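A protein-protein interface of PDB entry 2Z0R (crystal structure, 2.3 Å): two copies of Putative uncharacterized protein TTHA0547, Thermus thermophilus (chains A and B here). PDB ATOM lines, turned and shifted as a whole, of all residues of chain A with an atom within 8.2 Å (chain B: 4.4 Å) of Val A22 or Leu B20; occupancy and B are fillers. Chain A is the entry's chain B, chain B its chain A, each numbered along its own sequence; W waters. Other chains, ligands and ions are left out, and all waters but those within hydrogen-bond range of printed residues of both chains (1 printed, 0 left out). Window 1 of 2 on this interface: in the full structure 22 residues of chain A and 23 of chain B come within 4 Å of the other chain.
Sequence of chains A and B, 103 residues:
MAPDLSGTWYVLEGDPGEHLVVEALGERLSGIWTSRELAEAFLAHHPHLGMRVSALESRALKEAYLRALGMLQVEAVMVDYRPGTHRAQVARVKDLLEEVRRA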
ATOM      1  N   HIS A  19      -3.226  25.899 -37.817  1.00  0.00           N
ATOM      2  CA  HIS A  19      -2.763  25.392 -36.541  1.00  0.00           C
ATOM      3  C   HIS A  19      -3.761  24.410 -35.952  1.00  0.00           C
ATOM      4  O   HIS A  19      -4.933  24.408 -36.303  1.00  0.00           O
ATOM      5  CB  HIS A  19      -2.526  26.552 -35.577  1.00  0.00           C
ATOM      6  CG  HIS A  19      -1.536  27.553 -36.083  1.00  0.00           C
ATOM      7  ND1 HIS A  19      -1.911  28.770 -36.611  1.00  0.00           N
ATOM      8  CD2 HIS A  19      -0.185  27.495 -36.186  1.00  0.00           C
ATOM      9  CE1 HIS A  19      -0.834  29.419 -37.019  1.00  0.00           C
ATOM     10  NE2 HIS A  19       0.226  28.667 -36.773  1.00  0.00           N
ATOM     11  N   LEU A  20      -3.282  23.569 -35.054  1.00  0.00           N
ATOM     12  CA  LEU A  20      -4.140  22.584 -34.434  1.00  0.00           C
ATOM     13  C   LEU A  20      -5.137  23.212 -33.475  1.00  0.00           C
ATOM     14  O   LEU A  20      -4.744  23.885 -32.536  1.00  0.00           O
ATOM     15  CB  LEU A  20      -3.306  21.567 -33.659  1.00  0.00           C
ATOM     16  CG  LEU A  20      -4.147  20.519 -32.932  1.00  0.00           C
ATOM     17  CD1 LEU A  20      -4.538  19.440 -33.913  1.00  0.00           C
ATOM     18  CD2 LEU A  20      -3.358  19.930 -31.774  1.00  0.00           C
ATOM     19  N   VAL A  21      -6.422  22.999 -33.723  1.00  0.00           N
ATOM     20  CA  VAL A  21      -7.452  23.499 -32.826  1.00  0.00           C
ATOM     21  C   VAL A  21      -8.210  22.269 -32.346  1.00  0.00           C
ATOM     22  O   VAL A  21      -8.574  21.407 -33.143  1.00  0.00           O
ATOM     23  CB  VAL A  21      -8.451  24.451 -33.528  1.00  0.00           C
ATOM     24  CG1 VAL A  21      -9.588  24.781 -32.583  1.00  0.00           C
ATOM     25  CG2 VAL A  21      -7.750  25.735 -33.952  1.00  0.00           C
ATOM     26  N   VAL A  22      -8.428  22.176 -31.041  1.00  0.00           N
ATOM     27  CA  VAL A  22      -9.148  21.049 -30.482  1.00  0.00           C
ATOM     28  C   VAL A  22     -10.337  21.549 -29.662  1.00  0.00           C
ATOM     29  O   VAL A  22     -10.223  22.521 -28.921  1.00  0.00           O
ATOM     30  CB  VAL A  22      -8.230  20.209 -29.577  1.00  0.00           C
ATOM     31  CG1 VAL A  22      -8.926  18.918 -29.181  1.00  0.00           C
ATOM     32  CG2 VAL A  22      -6.926  19.921 -30.297  1.00  0.00           C
ATOM     33  N   GLU A  23     -11.484  20.897 -29.800  1.00  0.00           N
ATOM     34  CA  GLU A  23     -12.643  21.314 -29.030  1.00  0.00           C
ATOM     35  C   GLU A  23     -12.892  20.402 -27.849  1.00  0.00           C
ATOM     36  O   GLU A  23     -13.283  19.253 -28.000  1.00  0.00           O
ATOM     37  CB  GLU A  23     -13.878  21.398 -29.919  1.00  0.00           C
ATOM     38  CG  GLU A  23     -13.764  22.562 -30.888  1.00  0.00           C
ATOM     39  CD  GLU A  23     -14.969  22.717 -31.770  1.00  0.00           C
ATOM     40  OE1 GLU A  23     -15.874  21.852 -31.695  1.00  0.00           O
ATOM     41  OE2 GLU A  23     -15.001  23.702 -32.541  1.00  0.00           O
ATOM     42  N   ALA A  24     -12.629  20.939 -26.662  1.00  0.00           N
ATOM     43  CA  ALA A  24     -12.816  20.219 -25.417  1.00  0.00           C
ATOM     44  C   ALA A  24     -12.957  21.276 -24.333  1.00  0.00           C
ATOM     45  O   ALA A  24     -12.610  22.438 -24.550  1.00  0.00           O
ATOM     46  CB  ALA A  24     -11.613  19.338 -25.143  1.00  0.00           C
ATOM     47  N   LEU A  25     -13.466  20.879 -23.173  1.00  0.00           N
ATOM     48  CA  LEU A  25     -13.647  21.805 -22.058  1.00  0.00           C
ATOM     49  C   LEU A  25     -14.577  22.951 -22.436  1.00  0.00           C
ATOM     50  O   LEU A  25     -14.477  24.052 -21.891  1.00  0.00           O
ATOM     51  CB  LEU A  25     -12.288  22.356 -21.614  1.00  0.00           C
ATOM     52  CG  LEU A  25     -11.243  21.255 -21.410  1.00  0.00           C
ATOM     53  CD1 LEU A  25      -9.967  21.864 -20.873  1.00  0.00           C
ATOM     54  CD2 LEU A  25     -11.784  20.200 -20.442  1.00  0.00           C
ATOM     55  N   GLY A  26     -15.478  22.680 -23.377  1.00  0.00           N
ATOM     56  CA  GLY A  26     -16.436  23.678 -23.824  1.00  0.00           C
ATOM     57  C   GLY A  26     -15.826  24.861 -24.552  1.00  0.00           C
ATOM     58  O   GLY A  26     -16.372  25.958 -24.531  1.00  0.00           O
ATOM     59  N   GLU A  27     -14.697  24.652 -25.215  1.00  0.00           N
ATOM     60  CA  GLU A  27     -14.065  25.754 -25.926  1.00  0.00           C
ATOM     61  C   GLU A  27     -13.190  25.270 -27.057  1.00  0.00           C
ATOM     62  O   GLU A  27     -13.018  24.066 -27.253  1.00  0.00           O
ATOM     63  CB  GLU A  27     -13.228  26.580 -24.948  1.00  0.00           C
ATOM     64  CG  GLU A  27     -12.672  27.865 -25.531  1.00  0.00           C
ATOM     65  CD  GLU A  27     -12.129  28.791 -24.462  1.00  0.00           C
ATOM     66  OE1 GLU A  27     -11.705  29.916 -24.817  1.00  0.00           O
ATOM     67  OE2 GLU A  27     -12.128  28.392 -23.271  1.00  0.00           O
ATOM     68  N   ARG A  28     -12.669  26.217 -27.819  1.00  0.00           N
ATOM     69  CA  ARG A  28     -11.769  25.909 -28.912  1.00  0.00           C
ATOM     70  C   ARG A  28     -10.368  26.137 -28.345  1.00  0.00           C
ATOM     71  O   ARG A  28     -10.025  27.255 -27.951  1.00  0.00           O
ATOM     72  CB  ARG A  28     -12.053  26.826 -30.104  1.00  0.00           C
ATOM     73  CG  ARG A  28     -13.307  26.413 -30.885  1.00  0.00           C
ATOM     74  CD  ARG A  28     -13.762  27.466 -31.897  1.00  0.00           C
ATOM     75  NE  ARG A  28     -12.823  27.687 -32.998  1.00  0.00           N
ATOM     76  CZ  ARG A  28     -12.510  26.772 -33.917  1.00  0.00           C
ATOM     77  NH1 ARG A  28     -13.052  25.567 -33.867  1.00  0.00           N
ATOM     78  NH2 ARG A  28     -11.677  27.076 -34.907  1.00  0.00           N
ATOM     79  N   LEU A  29      -9.579  25.064 -28.281  1.00  0.00           N
ATOM     80  CA  LEU A  29      -8.231  25.128 -27.738  1.00  0.00           C
ATOM     81  C   LEU A  29      -7.142  24.842 -28.761  1.00  0.00           C
ATOM     82  O   LEU A  29      -7.343  24.078 -29.711  1.00  0.00           O
ATOM     83  CB  LEU A  29      -8.065  24.105 -26.597  1.00  0.00           C
ATOM     84  CG  LEU A  29      -9.074  24.063 -25.442  1.00  0.00           C
ATOM     85  CD1 LEU A  29      -8.939  22.743 -24.709  1.00  0.00           C
ATOM     86  CD2 LEU A  29      -8.862  25.244 -24.496  1.00  0.00           C
ATOM     87  N   SER A  30      -5.987  25.471 -28.566  1.00  0.00           N
ATOM     88  CA  SER A  30      -4.833  25.205 -29.413  1.00  0.00           C
ATOM     89  C   SER A  30      -3.744  24.781 -28.421  1.00  0.00           C
ATOM     90  O   SER A  30      -4.035  24.475 -27.263  1.00  0.00           O
ATOM     91  CB  SER A  30      -4.390  26.448 -30.176  1.00  0.00           C
ATOM     92  OG  SER A  30      -3.312  26.126 -31.045  1.00  0.00           O
ATOM     93  N   GLY A  31      -2.494  24.768 -28.849  1.00  0.00           N
ATOM     94  CA  GLY A  31      -1.470  24.362 -27.921  1.00  0.00           C
ATOM     95  C   GLY A  31      -0.145  25.051 -28.104  1.00  0.00           C
ATOM     96  O   GLY A  31       0.227  25.441 -29.213  1.00  0.00           O
ATOM     97  N   TRP A  33       3.911  24.558 -26.601  1.00  0.00           N
ATOM     98  CA  TRP A  33       4.830  23.739 -25.827  1.00  0.00           C
ATOM     99  C   TRP A  33       6.067  24.587 -25.563  1.00  0.00           C
ATOM    100  O   TRP A  33       6.467  25.390 -26.412  1.00  0.00           O
ATOM    101  CB  TRP A  33       5.163  22.449 -26.584  1.00  0.00           C
ATOM    102  CG  TRP A  33       4.015  21.473 -26.530  1.00  0.00           C
ATOM    103  CD1 TRP A  33       3.790  20.534 -25.567  1.00  0.00           C
ATOM    104  CD2 TRP A  33       2.890  21.411 -27.423  1.00  0.00           C
ATOM    105  NE1 TRP A  33       2.594  19.895 -25.798  1.00  0.00           N
ATOM    106  CE2 TRP A  33       2.022  20.412 -26.931  1.00  0.00           C
ATOM    107  CE3 TRP A  33       2.531  22.106 -28.590  1.00  0.00           C
ATOM    108  CZ2 TRP A  33       0.812  20.085 -27.563  1.00  0.00           C
ATOM    109  CZ3 TRP A  33       1.321  21.782 -29.224  1.00  0.00           C
ATOM    110  CH2 TRP A  33       0.479  20.778 -28.706  1.00  0.00           C
ATOM    111  N   PHE A  42       4.518  15.235 -28.234  1.00  0.00           N
ATOM    112  CA  PHE A  42       3.082  15.275 -28.479  1.00  0.00           C
ATOM    113  C   PHE A  42       2.815  14.933 -29.945  1.00  0.00           C
ATOM    114  O   PHE A  42       1.873  14.206 -30.270  1.00  0.00           O
ATOM    115  CB  PHE A  42       2.514  16.662 -28.171  1.00  0.00           C
ATOM    116  CG  PHE A  42       1.066  16.811 -28.543  1.00  0.00           C
ATOM    117  CD1 PHE A  42       0.065  16.415 -27.669  1.00  0.00           C
ATOM    118  CD2 PHE A  42       0.702  17.316 -29.789  1.00  0.00           C
ATOM    119  CE1 PHE A  42      -1.281  16.519 -28.027  1.00  0.00           C
ATOM    120  CE2 PHE A  42      -0.644  17.422 -30.156  1.00  0.00           C
ATOM    121  CZ  PHE A  42      -1.637  17.023 -29.272  1.00  0.00           C
ATOM    122  N   HIS A  46       0.409  11.888 -32.099  1.00  0.00           N
ATOM    123  CA  HIS A  46      -0.727  12.313 -32.918  1.00  0.00           C
ATOM    124  C   HIS A  46      -0.361  12.456 -34.392  1.00  0.00           C
ATOM    125  O   HIS A  46      -0.295  13.560 -34.923  1.00  0.00           O
ATOM    126  CB  HIS A  46      -1.306  13.630 -32.399  1.00  0.00           C
ATOM    127  CG  HIS A  46      -1.747  13.555 -30.975  1.00  0.00           C
ATOM    128  ND1 HIS A  46      -0.858  13.606 -29.922  1.00  0.00           N
ATOM    129  CD2 HIS A  46      -2.959  13.287 -30.433  1.00  0.00           C
ATOM    130  CE1 HIS A  46      -1.500  13.359 -28.795  1.00  0.00           C
ATOM    131  NE2 HIS A  46      -2.776  13.160 -29.078  1.00  0.00           N
ATOM    132  N   LEU A  49      -2.237  13.860 -38.916  1.00  0.00           N
ATOM    133  CA  LEU A  49      -2.973  15.112 -38.801  1.00  0.00           C
ATOM    134  C   LEU A  49      -2.310  16.171 -39.672  1.00  0.00           C
ATOM    135  O   LEU A  49      -2.711  17.333 -39.655  1.00  0.00           O
ATOM    136  CB  LEU A  49      -3.009  15.589 -37.343  1.00  0.00           C
ATOM    137  CG  LEU A  49      -3.823  14.713 -36.384  1.00  0.00           C
ATOM    138  CD1 LEU A  49      -3.680  15.233 -34.957  1.00  0.00           C
ATOM    139  CD2 LEU A  49      -5.301  14.696 -36.817  1.00  0.00           C
ATOM    140  N   VAL A  74     -10.063  31.033 -31.189  1.00  0.00           N
ATOM    141  CA  VAL A  74      -9.578  30.201 -30.104  1.00  0.00           C
ATOM    142  C   VAL A  74      -9.324  31.172 -28.949  1.00  0.00           C
ATOM    143  O   VAL A  74      -8.621  32.158 -29.113  1.00  0.00           O
ATOM    144  CB  VAL A  74      -8.269  29.488 -30.526  1.00  0.00           C
ATOM    145  CG1 VAL A  74      -7.675  28.735 -29.364  1.00  0.00           C
ATOM    146  CG2 VAL A  74      -8.555  28.543 -31.693  1.00  0.00           C
ATOM    147  N   ALA A  76      -8.253  30.064 -25.796  1.00  0.00           N
ATOM    148  CA  ALA A  76      -7.420  29.421 -24.788  1.00  0.00           C
ATOM    149  C   ALA A  76      -6.468  28.432 -25.425  1.00  0.00           C
ATOM    150  O   ALA A  76      -6.763  27.866 -26.472  1.00  0.00           O
ATOM    151  CB  ALA A  76      -8.294  28.710 -23.753  1.00  0.00           C
ATOM    152  N   MET A  78      -3.547  25.206 -24.365  1.00  0.00           N
ATOM    153  CA  MET A  78      -3.046  24.363 -23.309  1.00  0.00           C
ATOM    154  C   MET A  78      -1.544  24.438 -23.423  1.00  0.00           C
ATOM    155  O   MET A  78      -0.993  24.350 -24.520  1.00  0.00           O
ATOM    156  CB  MET A  78      -3.569  22.947 -23.464  1.00  0.00           C
ATOM    157  CG  MET A  78      -5.062  22.906 -23.227  1.00  0.00           C
ATOM    158  SD  MET A  78      -5.737  21.173 -22.815  1.00  0.00           S
ATOM    159  CE  MET A  78      -5.763  20.487 -24.629  1.00  0.00           C
ATOM    160  N   TYR A  81       0.964  20.477 -22.858  1.00  0.00           N
ATOM    161  CA  TYR A  81       0.047  19.379 -22.637  1.00  0.00           C
ATOM    162  C   TYR A  81       0.755  18.042 -22.878  1.00  0.00           C
ATOM    163  O   TYR A  81       1.576  17.905 -23.792  1.00  0.00           O
ATOM    164  CB  TYR A  81      -1.142  19.473 -23.581  1.00  0.00           C
ATOM    165  CG  TYR A  81      -2.133  18.343 -23.408  1.00  0.00           C
ATOM    166  CD1 TYR A  81      -3.142  18.415 -22.444  1.00  0.00           C
ATOM    167  CD2 TYR A  81      -2.063  17.195 -24.207  1.00  0.00           C
ATOM    168  CE1 TYR A  81      -4.061  17.380 -22.278  1.00  0.00           C
ATOM    169  CE2 TYR A  81      -2.977  16.150 -24.049  1.00  0.00           C
ATOM    170  CZ  TYR A  81      -3.975  16.252 -23.083  1.00  0.00           C
ATOM    171  OH  TYR A  81      -4.896  15.238 -22.932  1.00  0.00           O
ATOM    172  N   LEU B  12     -16.197   9.201 -27.624  1.00  0.00           N
ATOM    173  CA  LEU B  12     -15.874  10.028 -26.474  1.00  0.00           C
ATOM    174  C   LEU B  12     -16.989  11.048 -26.254  1.00  0.00           C
ATOM    175  O   LEU B  12     -17.556  11.585 -27.207  1.00  0.00           O
ATOM    176  CB  LEU B  12     -14.552  10.770 -26.701  1.00  0.00           C
ATOM    177  CG  LEU B  12     -13.303   9.897 -26.834  1.00  0.00           C
ATOM    178  CD1 LEU B  12     -12.104  10.776 -27.144  1.00  0.00           C
ATOM    179  CD2 LEU B  12     -13.081   9.108 -25.536  1.00  0.00           C
ATOM    180  N   HIS B  19     -18.091  16.439 -28.322  1.00  0.00           N
ATOM    181  CA  HIS B  19     -17.271  15.296 -28.608  1.00  0.00           C
ATOM    182  C   HIS B  19     -15.923  15.950 -28.868  1.00  0.00           C
ATOM    183  O   HIS B  19     -15.810  17.192 -28.883  1.00  0.00           O
ATOM    184  CB  HIS B  19     -17.810  14.537 -29.824  1.00  0.00           C
ATOM    185  CG  HIS B  19     -19.212  14.046 -29.640  1.00  0.00           C
ATOM    186  ND1 HIS B  19     -20.300  14.655 -30.229  1.00  0.00           N
ATOM    187  CD2 HIS B  19     -19.713  13.056 -28.859  1.00  0.00           C
ATOM    188  CE1 HIS B  19     -21.409  14.066 -29.816  1.00  0.00           C
ATOM    189  NE2 HIS B  19     -21.081  13.092 -28.983  1.00  0.00           N
ATOM    190  N   LEU B  20     -14.897  15.134 -29.035  1.00  0.00           N
ATOM    191  CA  LEU B  20     -13.576  15.667 -29.262  1.00  0.00           C
ATOM    192  C   LEU B  20     -13.488  15.954 -30.747  1.00  0.00           C
ATOM    193  O   LEU B  20     -13.505  15.031 -31.556  1.00  0.00           O
ATOM    194  CB  LEU B  20     -12.532  14.625 -28.852  1.00  0.00           C
ATOM    195  CG  LEU B  20     -11.066  15.031 -28.748  1.00  0.00           C
ATOM    196  CD1 LEU B  20     -10.904  16.102 -27.671  1.00  0.00           C
ATOM    197  CD2 LEU B  20     -10.230  13.803 -28.406  1.00  0.00           C
ATOM    198  N   VAL B  21     -13.447  17.230 -31.111  1.00  0.00           N
ATOM    199  CA  VAL B  21     -13.316  17.605 -32.516  1.00  0.00           C
ATOM    200  C   VAL B  21     -11.960  18.257 -32.682  1.00  0.00           C
ATOM    201  O   VAL B  21     -11.524  19.041 -31.828  1.00  0.00           O
ATOM    202  CB  VAL B  21     -14.413  18.609 -32.983  1.00  0.00           C
ATOM    203  CG1 VAL B  21     -14.107  19.111 -34.408  1.00  0.00           C
ATOM    204  CG2 VAL B  21     -15.768  17.938 -32.971  1.00  0.00           C
ATOM    205  N   VAL B  22     -11.278  17.909 -33.764  1.00  0.00           N
ATOM    206  CA  VAL B  22      -9.977  18.493 -34.046  1.00  0.00           C
ATOM    207  C   VAL B  22      -9.966  19.073 -35.449  1.00  0.00           C
ATOM    208  O   VAL B  22     -10.544  18.496 -36.371  1.00  0.00           O
ATOM    209  CB  VAL B  22      -8.835  17.444 -33.930  1.00  0.00           C
ATOM    210  CG1 VAL B  22      -9.030  16.329 -34.935  1.00  0.00           C
ATOM    211  CG2 VAL B  22      -7.490  18.112 -34.167  1.00  0.00           C
ATOM    212  N   LEU B  29     -12.841  17.136 -37.644  1.00  0.00           N
ATOM    213  CA  LEU B  29     -12.900  15.696 -37.448  1.00  0.00           C
ATOM    214  C   LEU B  29     -13.129  15.271 -36.009  1.00  0.00           C
ATOM    215  O   LEU B  29     -12.771  15.979 -35.070  1.00  0.00           O
ATOM    216  CB  LEU B  29     -11.586  15.052 -37.905  1.00  0.00           C
ATOM    217  CG  LEU B  29     -10.980  15.367 -39.273  1.00  0.00           C
ATOM    218  CD1 LEU B  29      -9.456  15.185 -39.209  1.00  0.00           C
ATOM    219  CD2 LEU B  29     -11.586  14.464 -40.314  1.00  0.00           C
ATOM    220  N   SER B  30     -13.711  14.088 -35.853  1.00  0.00           N
ATOM    221  CA  SER B  30     -13.922  13.517 -34.542  1.00  0.00           C
ATOM    222  C   SER B  30     -13.372  12.092 -34.604  1.00  0.00           C
ATOM    223  O   SER B  30     -12.674  11.733 -35.553  1.00  0.00           O
ATOM    224  CB  SER B  30     -15.406  13.492 -34.179  1.00  0.00           C
ATOM    225  OG  SER B  30     -15.546  13.183 -32.802  1.00  0.00           O
ATOM    226  N   GLY B  31     -13.686  11.278 -33.605  1.00  0.00           N
ATOM    227  CA  GLY B  31     -13.183   9.917 -33.612  1.00  0.00           C
ATOM    228  C   GLY B  31     -14.169   8.857 -33.157  1.00  0.00           C
ATOM    229  O   GLY B  31     -14.968   9.062 -32.240  1.00  0.00           O
ATOM    230  N   PHE B  42      -6.887   5.414 -25.761  1.00  0.00           N
ATOM    231  CA  PHE B  42      -6.750   6.781 -26.251  1.00  0.00           C
ATOM    232  C   PHE B  42      -7.137   7.750 -25.134  1.00  0.00           C
ATOM    233  O   PHE B  42      -6.462   8.751 -24.891  1.00  0.00           O
ATOM    234  CB  PHE B  42      -7.670   7.021 -27.445  1.00  0.00           C
ATOM    235  CG  PHE B  42      -7.701   8.456 -27.904  1.00  0.00           C
ATOM    236  CD1 PHE B  42      -6.789   8.925 -28.857  1.00  0.00           C
ATOM    237  CD2 PHE B  42      -8.632   9.347 -27.379  1.00  0.00           C
ATOM    238  CE1 PHE B  42      -6.809  10.257 -29.281  1.00  0.00           C
ATOM    239  CE2 PHE B  42      -8.654  10.685 -27.799  1.00  0.00           C
ATOM    240  CZ  PHE B  42      -7.742  11.136 -28.751  1.00  0.00           C
ATOM    241  N   LEU B  49      -9.387  16.478 -20.344  1.00  0.00           N
ATOM    242  CA  LEU B  49     -10.275  16.949 -21.406  1.00  0.00           C
ATOM    243  C   LEU B  49     -11.730  16.682 -21.035  1.00  0.00           C
ATOM    244  O   LEU B  49     -12.637  16.912 -21.843  1.00  0.00           O
ATOM    245  CB  LEU B  49      -9.930  16.261 -22.732  1.00  0.00           C
ATOM    246  CG  LEU B  49      -8.484  16.449 -23.222  1.00  0.00           C
ATOM    247  CD1 LEU B  49      -8.240  15.611 -24.479  1.00  0.00           C
ATOM    248  CD2 LEU B  49      -8.209  17.927 -23.492  1.00  0.00           C
ATOM    249  N   MET B  51     -13.316  14.004 -20.798  1.00  0.00           N
ATOM    250  CA  MET B  51     -13.962  13.009 -21.646  1.00  0.00           C
ATOM    251  C   MET B  51     -14.154  11.636 -20.998  1.00  0.00           C
ATOM    252  O   MET B  51     -13.517  11.304 -19.998  1.00  0.00           O
ATOM    253  CB  MET B  51     -13.150  12.848 -22.936  1.00  0.00           C
ATOM    254  CG  MET B  51     -13.015  14.121 -23.785  1.00  0.00           C
ATOM    255  SD  MET B  51     -14.649  14.593 -24.724  1.00  0.00           S
ATOM    256  CE  MET B  51     -14.367  16.481 -25.031  1.00  0.00           C
HETATM  257  O   HOH W   1     -17.247  20.097 -30.169  1.00  0.00           O
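N of Glu A23 is in hydrogen-bond range of O of Val B21 (2.7 Å).
The backbone carbonyl oxygen of Glu A23 lies close to the backbone carbonyl oxygen of His B19, 3.4 Å away.
The side-chain hydroxyl of Ser B30 lies within hydrogen-bond range of the backbone carbonyl oxygen of Leu B20 (3.0 Å).
The backbone carbonyl oxygen (O) of Leu B29 is in hydrogen-bond range of the backbone NH (N) of Val B22, 2.8 Å away.
O of Leu A20 is in hydrogen-bond range of OG of Ser A30, 3.0 Å away.
The guanidinium group (NH1) of Arg A28 lies within salt-bridge range of the side-chain carboxylate (OE2) of Glu A23.
The backbone carbonyl oxygen of Ser A30 is in hydrogen-bond range of the backbone NH of Met A78, at 3.0 Å.
The indole nitrogen (NE1) of Trp A33 lies within hydrogen-bond range of the backbone carbonyl oxygen (O) of Tyr A81 (3.0 Å).
Among the printed residues, merely in contact across the chains: Leu A20 with Val B22, Val A21 with Val B22, Val A22 with Val B21, Leu A25 with Leu B49, Tyr A81 with Leu B49, Met A78 with Leu B49, Val A22 with Leu B20, Glu A23 with Leu B20 and Ala A24 with Met B51.
Of the printed residues of chain B, Leu A20 touches Val B22.
Of the printed residues of chain B, Ala A24 touches Met B51 (3.97 Å).
Of chain A, only Val A22 and Glu A23 come within 4 Å of Leu B20.
Ser B30 touches none of the printed residues of chain A.
Printed residues of chain A within 4 Å of Met B51: Ala A24 (3.97 Å).
The nearest residue of chain B that does not touch Val A22 is Val B22 (4.3 Å).
The nearest residue of chain A that does not touch Leu B20 is Ala A24 (4.2 Å).
Of the 21 printed residues of chain A, 8 touch a printed residue of chain B.
Hydrophobic or aromatic side chains of chain A within 4 Å of the printed part of chain B: Leu A20, Val A22, Ala A24, Leu A25, Met A78 and Tyr A81.
Of the 11 printed residues of chain B, 6 touch a printed residue of chain A.
Hydrophobic or aromatic side chains of chain B that line the printed part of chain A: Leu B20, Val B21, Val B22, Leu B49 and Met B51.
Leu A20 touches Val B22, and with the chains exchanged Val A22 touches Leu B20.
Val A21 touches Val B22, and with the chains exchanged Val A22 touches Val B21.
Positions printed for both chains: 19, 20, 21, 22, 29, 30, 31, 42 and 49.
Water W1 lies within hydrogen-bond range of OE1 of Glu A23 (2.7 Å) and O of His B19 (3.5 Å).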
